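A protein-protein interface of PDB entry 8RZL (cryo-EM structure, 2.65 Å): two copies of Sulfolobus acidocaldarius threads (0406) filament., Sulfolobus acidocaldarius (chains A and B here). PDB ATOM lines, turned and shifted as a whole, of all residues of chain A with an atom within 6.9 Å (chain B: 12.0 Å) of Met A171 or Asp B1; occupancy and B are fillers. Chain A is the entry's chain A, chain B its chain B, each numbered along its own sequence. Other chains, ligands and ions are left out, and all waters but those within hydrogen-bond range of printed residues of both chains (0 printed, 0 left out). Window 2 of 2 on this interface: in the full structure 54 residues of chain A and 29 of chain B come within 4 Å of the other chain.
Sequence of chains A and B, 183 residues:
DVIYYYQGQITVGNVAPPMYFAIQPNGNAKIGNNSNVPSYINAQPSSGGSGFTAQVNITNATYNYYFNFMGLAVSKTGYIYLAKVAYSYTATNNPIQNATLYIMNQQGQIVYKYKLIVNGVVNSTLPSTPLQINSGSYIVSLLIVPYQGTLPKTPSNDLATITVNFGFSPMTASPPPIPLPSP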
ATOM      1  N   THR A  77     -18.128 -13.220  13.012  1.00  0.00           N
ATOM      2  CA  THR A  77     -19.087 -12.227  13.497  1.00  0.00           C
ATOM      3  C   THR A  77     -18.540 -11.491  14.721  1.00  0.00           C
ATOM      4  O   THR A  77     -17.792 -12.065  15.512  1.00  0.00           O
ATOM      5  CB  THR A  77     -20.464 -12.834  13.811  1.00  0.00           C
ATOM      6  OG1 THR A  77     -20.360 -13.693  14.948  1.00  0.00           O
ATOM      7  CG2 THR A  77     -21.068 -13.606  12.659  1.00  0.00           C
ATOM      8  N   GLY A  78     -18.923 -10.216  14.873  1.00  0.00           N
ATOM      9  CA  GLY A  78     -18.442  -9.389  15.968  1.00  0.00           C
ATOM     10  C   GLY A  78     -19.131  -8.029  15.991  1.00  0.00           C
ATOM     11  O   GLY A  78     -20.065  -7.805  15.236  1.00  0.00           O
ATOM     12  N   TYR A  79     -18.667  -7.137  16.873  1.00  0.00           N
ATOM     13  CA  TYR A  79     -19.256  -5.816  17.040  1.00  0.00           C
ATOM     14  C   TYR A  79     -18.265  -4.750  16.584  1.00  0.00           C
ATOM     15  O   TYR A  79     -17.117  -4.760  17.014  1.00  0.00           O
ATOM     16  CB  TYR A  79     -19.701  -5.597  18.491  1.00  0.00           C
ATOM     17  CG  TYR A  79     -20.766  -6.561  18.949  1.00  0.00           C
ATOM     18  CD1 TYR A  79     -20.433  -7.836  19.390  1.00  0.00           C
ATOM     19  CD2 TYR A  79     -22.111  -6.224  18.908  1.00  0.00           C
ATOM     20  CE1 TYR A  79     -21.402  -8.752  19.766  1.00  0.00           C
ATOM     21  CE2 TYR A  79     -23.095  -7.128  19.292  1.00  0.00           C
ATOM     22  CZ  TYR A  79     -22.741  -8.400  19.719  1.00  0.00           C
ATOM     23  OH  TYR A  79     -23.698  -9.297  20.109  1.00  0.00           O
ATOM     24  N   GLN A 132     -23.563  -5.063  15.899  1.00  0.00           N
ATOM     25  CA  GLN A 132     -23.169  -6.348  15.337  1.00  0.00           C
ATOM     26  C   GLN A 132     -22.985  -6.258  13.821  1.00  0.00           C
ATOM     27  O   GLN A 132     -23.786  -5.632  13.138  1.00  0.00           O
ATOM     28  CB  GLN A 132     -24.211  -7.413  15.673  1.00  0.00           C
ATOM     29  CG  GLN A 132     -23.776  -8.811  15.258  1.00  0.00           C
ATOM     30  CD  GLN A 132     -24.740  -9.896  15.671  1.00  0.00           C
ATOM     31  OE1 GLN A 132     -24.411 -10.780  16.464  1.00  0.00           O
ATOM     32  NE2 GLN A 132     -25.947  -9.845  15.128  1.00  0.00           N
ATOM     33  N   PHE A 168     -13.133  -3.045  16.341  1.00  0.00           N
ATOM     34  CA  PHE A 168     -13.872  -4.280  16.142  1.00  0.00           C
ATOM     35  C   PHE A 168     -13.552  -5.224  17.297  1.00  0.00           C
ATOM     36  O   PHE A 168     -12.395  -5.333  17.693  1.00  0.00           O
ATOM     37  CB  PHE A 168     -13.496  -4.913  14.801  1.00  0.00           C
ATOM     38  CG  PHE A 168     -14.217  -6.200  14.482  1.00  0.00           C
ATOM     39  CD1 PHE A 168     -13.811  -7.402  15.044  1.00  0.00           C
ATOM     40  CD2 PHE A 168     -15.298  -6.212  13.611  1.00  0.00           C
ATOM     41  CE1 PHE A 168     -14.490  -8.581  14.768  1.00  0.00           C
ATOM     42  CE2 PHE A 168     -15.960  -7.396  13.311  1.00  0.00           C
ATOM     43  CZ  PHE A 168     -15.553  -8.578  13.892  1.00  0.00           C
ATOM     44  N   SER A 169     -14.573  -5.922  17.810  1.00  0.00           N
ATOM     45  CA  SER A 169     -14.368  -6.914  18.854  1.00  0.00           C
ATOM     46  C   SER A 169     -15.022  -8.238  18.463  1.00  0.00           C
ATOM     47  O   SER A 169     -16.193  -8.264  18.094  1.00  0.00           O
ATOM     48  CB  SER A 169     -14.870  -6.407  20.173  1.00  0.00           C
ATOM     49  OG  SER A 169     -16.252  -6.129  20.094  1.00  0.00           O
ATOM     50  N   PRO A 170     -14.287  -9.375  18.517  1.00  0.00           N
ATOM     51  CA  PRO A 170     -14.828 -10.669  18.090  1.00  0.00           C
ATOM     52  C   PRO A 170     -15.639 -11.415  19.154  1.00  0.00           C
ATOM     53  O   PRO A 170     -15.836 -12.624  19.049  1.00  0.00           O
ATOM     54  CB  PRO A 170     -13.542 -11.428  17.733  1.00  0.00           C
ATOM     55  CG  PRO A 170     -12.545 -10.926  18.753  1.00  0.00           C
ATOM     56  CD  PRO A 170     -12.876  -9.460  18.931  1.00  0.00           C
ATOM     57  N   MET A 171     -16.143 -10.690  20.158  1.00  0.00           N
ATOM     58  CA  MET A 171     -16.897 -11.286  21.254  1.00  0.00           C
ATOM     59  C   MET A 171     -18.338 -11.603  20.840  1.00  0.00           C
ATOM     60  O   MET A 171     -18.881 -10.998  19.915  1.00  0.00           O
ATOM     61  CB  MET A 171     -16.895 -10.357  22.472  1.00  0.00           C
ATOM     62  CG  MET A 171     -15.502 -10.025  22.972  1.00  0.00           C
ATOM     63  SD  MET A 171     -15.527  -9.045  24.500  1.00  0.00           S
ATOM     64  CE  MET A 171     -16.013 -10.289  25.695  1.00  0.00           C
ATOM     65  N   THR A 172     -18.966 -12.547  21.559  1.00  0.00           N
ATOM     66  CA  THR A 172     -20.356 -12.940  21.342  1.00  0.00           C
ATOM     67  C   THR A 172     -21.330 -11.883  21.866  1.00  0.00           C
ATOM     68  O   THR A 172     -22.382 -11.653  21.261  1.00  0.00           O
ATOM     69  CB  THR A 172     -20.655 -14.318  21.948  1.00  0.00           C
ATOM     70  OG1 THR A 172     -19.858 -14.482  23.125  1.00  0.00           O
ATOM     71  CG2 THR A 172     -20.381 -15.444  20.978  1.00  0.00           C
ATOM     72  N   ALA A 173     -20.967 -11.242  22.991  1.00  0.00           N
ATOM     73  CA  ALA A 173     -21.753 -10.188  23.625  1.00  0.00           C
ATOM     74  C   ALA A 173     -21.105  -8.818  23.416  1.00  0.00           C
ATOM     75  O   ALA A 173     -19.881  -8.683  23.436  1.00  0.00           O
ATOM     76  CB  ALA A 173     -21.944 -10.480  25.092  1.00  0.00           C
ATOM     77  N   SER A 174     -21.955  -7.796  23.253  1.00  0.00           N
ATOM     78  CA  SER A 174     -21.530  -6.437  22.939  1.00  0.00           C
ATOM     79  C   SER A 174     -20.653  -5.862  24.057  1.00  0.00           C
ATOM     80  O   SER A 174     -21.039  -5.917  25.223  1.00  0.00           O
ATOM     81  CB  SER A 174     -22.736  -5.566  22.703  1.00  0.00           C
ATOM     82  OG  SER A 174     -22.343  -4.250  22.354  1.00  0.00           O
ATOM     83  N   PRO A 175     -19.462  -5.275  23.755  1.00  0.00           N
ATOM     84  CA  PRO A 175     -18.648  -4.603  24.769  1.00  0.00           C
ATOM     85  C   PRO A 175     -19.176  -3.195  25.045  1.00  0.00           C
ATOM     86  O   PRO A 175     -20.067  -2.710  24.345  1.00  0.00           O
ATOM     87  CB  PRO A 175     -17.277  -4.515  24.076  1.00  0.00           C
ATOM     88  CG  PRO A 175     -17.624  -4.322  22.620  1.00  0.00           C
ATOM     89  CD  PRO A 175     -18.831  -5.214  22.425  1.00  0.00           C
ATOM     90  N   PRO A 176     -18.629  -2.466  26.046  1.00  0.00           N
ATOM     91  CA  PRO A 176     -18.853  -1.026  26.135  1.00  0.00           C
ATOM     92  C   PRO A 176     -18.122  -0.346  24.977  1.00  0.00           C
ATOM     93  O   PRO A 176     -17.240  -0.945  24.362  1.00  0.00           O
ATOM     94  CB  PRO A 176     -18.226  -0.616  27.477  1.00  0.00           C
ATOM     95  CG  PRO A 176     -17.945  -1.913  28.206  1.00  0.00           C
ATOM     96  CD  PRO A 176     -17.774  -2.964  27.132  1.00  0.00           C
ATOM     97  N   ILE A 178     -15.346   1.201  24.065  1.00  0.00           N
ATOM     98  CA  ILE A 178     -14.010   1.457  24.597  1.00  0.00           C
ATOM     99  C   ILE A 178     -13.260   2.463  23.715  1.00  0.00           C
ATOM    100  O   ILE A 178     -13.030   2.189  22.539  1.00  0.00           O
ATOM    101  CB  ILE A 178     -13.210   0.144  24.764  1.00  0.00           C
ATOM    102  CG1 ILE A 178     -13.950  -0.936  25.564  1.00  0.00           C
ATOM    103  CG2 ILE A 178     -11.826   0.416  25.337  1.00  0.00           C
ATOM    104  CD1 ILE A 178     -14.392  -0.524  26.957  1.00  0.00           C
ATOM    105  N   ASP B   1     -12.340  -7.521  27.792  1.00  0.00           N
ATOM    106  CA  ASP B   1     -12.784  -7.418  26.377  1.00  0.00           C
ATOM    107  C   ASP B   1     -11.571  -7.234  25.472  1.00  0.00           C
ATOM    108  O   ASP B   1     -10.570  -6.649  25.878  1.00  0.00           O
ATOM    109  CB  ASP B   1     -13.760  -6.254  26.187  1.00  0.00           C
ATOM    110  CG  ASP B   1     -14.966  -6.269  27.121  1.00  0.00           C
ATOM    111  OD1 ASP B   1     -15.029  -7.148  28.009  1.00  0.00           O
ATOM    112  OD2 ASP B   1     -15.835  -5.396  26.955  1.00  0.00           O
ATOM    113  N   VAL B   2     -11.674  -7.762  24.249  1.00  0.00           N
ATOM    114  CA  VAL B   2     -10.635  -7.590  23.245  1.00  0.00           C
ATOM    115  C   VAL B   2     -11.189  -6.727  22.118  1.00  0.00           C
ATOM    116  O   VAL B   2     -12.176  -7.089  21.480  1.00  0.00           O
ATOM    117  CB  VAL B   2     -10.107  -8.937  22.714  1.00  0.00           C
ATOM    118  CG1 VAL B   2      -9.005  -8.744  21.684  1.00  0.00           C
ATOM    119  CG2 VAL B   2      -9.622  -9.828  23.842  1.00  0.00           C
ATOM    120  N   ILE B   3     -10.535  -5.581  21.890  1.00  0.00           N
ATOM    121  CA  ILE B   3     -10.852  -4.700  20.777  1.00  0.00           C
ATOM    122  C   ILE B   3      -9.657  -4.663  19.827  1.00  0.00           C
ATOM    123  O   ILE B   3      -8.528  -4.407  20.244  1.00  0.00           O
ATOM    124  CB  ILE B   3     -11.224  -3.267  21.229  1.00  0.00           C
ATOM    125  CG1 ILE B   3     -12.096  -3.187  22.491  1.00  0.00           C
ATOM    126  CG2 ILE B   3     -11.800  -2.477  20.062  1.00  0.00           C
ATOM    127  CD1 ILE B   3     -13.490  -3.781  22.371  1.00  0.00           C
ATOM    128  N   TYR B   4      -9.932  -4.888  18.542  1.00  0.00           N
ATOM    129  CA  TYR B   4      -8.952  -4.671  17.493  1.00  0.00           C
ATOM    130  C   TYR B   4      -9.320  -3.383  16.766  1.00  0.00           C
ATOM    131  O   TYR B   4     -10.453  -3.244  16.313  1.00  0.00           O
ATOM    132  CB  TYR B   4      -8.893  -5.893  16.571  1.00  0.00           C
ATOM    133  CG  TYR B   4      -8.415  -7.153  17.248  1.00  0.00           C
ATOM    134  CD1 TYR B   4      -7.110  -7.264  17.710  1.00  0.00           C
ATOM    135  CD2 TYR B   4      -9.262  -8.237  17.439  1.00  0.00           C
ATOM    136  CE1 TYR B   4      -6.656  -8.416  18.337  1.00  0.00           C
ATOM    137  CE2 TYR B   4      -8.826  -9.394  18.072  1.00  0.00           C
ATOM    138  CZ  TYR B   4      -7.517  -9.487  18.519  1.00  0.00           C
ATOM    139  OH  TYR B   4      -7.079 -10.625  19.137  1.00  0.00           O
ATOM    140  N   TYR B   5      -8.363  -2.453  16.651  1.00  0.00           N
ATOM    141  CA  TYR B   5      -8.611  -1.191  15.973  1.00  0.00           C
ATOM    142  C   TYR B   5      -7.881  -1.133  14.632  1.00  0.00           C
ATOM    143  O   TYR B   5      -6.700  -1.472  14.538  1.00  0.00           O
ATOM    144  CB  TYR B   5      -8.198  -0.011  16.848  1.00  0.00           C
ATOM    145  CG  TYR B   5      -8.889   0.104  18.183  1.00  0.00           C
ATOM    146  CD1 TYR B   5     -10.077   0.807  18.319  1.00  0.00           C
ATOM    147  CD2 TYR B   5      -8.322  -0.431  19.329  1.00  0.00           C
ATOM    148  CE1 TYR B   5     -10.700   0.951  19.553  1.00  0.00           C
ATOM    149  CE2 TYR B   5      -8.921  -0.279  20.574  1.00  0.00           C
ATOM    150  CZ  TYR B   5     -10.121   0.407  20.688  1.00  0.00           C
ATOM    151  OH  TYR B   5     -10.732   0.556  21.905  1.00  0.00           O
ATOM    152  N   TYR B   6      -8.618  -0.672  13.612  1.00  0.00           N
ATOM    153  CA  TYR B   6      -8.156  -0.559  12.237  1.00  0.00           C
ATOM    154  C   TYR B   6      -8.189   0.913  11.839  1.00  0.00           C
ATOM    155  O   TYR B   6      -9.215   1.573  11.998  1.00  0.00           O
ATOM    156  CB  TYR B   6      -9.039  -1.406  11.314  1.00  0.00           C
ATOM    157  CG  TYR B   6      -9.132  -2.859  11.705  1.00  0.00           C
ATOM    158  CD1 TYR B   6      -9.942  -3.262  12.759  1.00  0.00           C
ATOM    159  CD2 TYR B   6      -8.408  -3.832  11.033  1.00  0.00           C
ATOM    160  CE1 TYR B   6     -10.020  -4.589  13.149  1.00  0.00           C
ATOM    161  CE2 TYR B   6      -8.483  -5.167  11.403  1.00  0.00           C
ATOM    162  CZ  TYR B   6      -9.297  -5.550  12.458  1.00  0.00           C
ATOM    163  OH  TYR B   6      -9.383  -6.862  12.835  1.00  0.00           O
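Of the 14 printed residues of chain A, 7 touch a printed residue of chain B. Along chain A the printed residues that touch a printed residue of chain B span positions 168 to 178. Among the printed residues, 10 pairs touch across the chains. Among the printed residues, no Asp or Glu carboxylate lies within 4 Å of a Lys or Arg side-chain nitrogen of the other chain.
The backbone carbonyl oxygen of Tyr A79 lies within hydrogen-bond range of the backbone NH of Ser A169 (2.9 Å).
No position is printed for both chains. Of the 10 pairs that touch across the chains among the printed residues, none has its exchanged pair printed and touching as well.
The side-chain hydroxyl (OH) of Tyr B5 lies within hydrogen-bond range of the backbone carbonyl oxygen (O) of Ile A178 (2.9 Å). The backbone NH of Tyr B4 is in hydrogen-bond range of the backbone carbonyl oxygen of Phe A168.
Thr A77 touches none of the printed residues of chain B. No residue of chain B comes within 4 Å of Gly A78. No residue of chain B comes within 4 Å of Tyr A79. Gln A132 touches none of the printed residues of chain B. Of the printed residues of chain B, Phe A168 touches Ile B3, Tyr B4 and Tyr B6. Of chain B, only Val B2 comes within 4 Å of Pro A170. Of chain B, only Asp B1 (3.7 Å) comes within 4 Å of Met A171. Of chain B, only Asp B1 comes within 4 Å of Pro A176. Of the printed residues of chain B, Ile A178 touches Tyr B5 (2.9 Å). Asp B1 touches three residues of chain A. Printed residues of chain A within 4 Å of Tyr B6: Phe A168.
Among the printed residues, pairs that only touch across the chains: Phe A168 with Ile B3 (3.5 Å), Phe A168 with Tyr B6 (3.9 Å), Ser A169 with Val B2 (3.1 Å), Ser A169 with Ile B3 (3.7 Å), Pro A170 with Val B2 (3.6 Å), Met A171 with Asp B1 (3.7 Å), Pro A175 with Asp B1 (3.3 Å) and Pro A176 with Asp B1 (3.1 Å).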
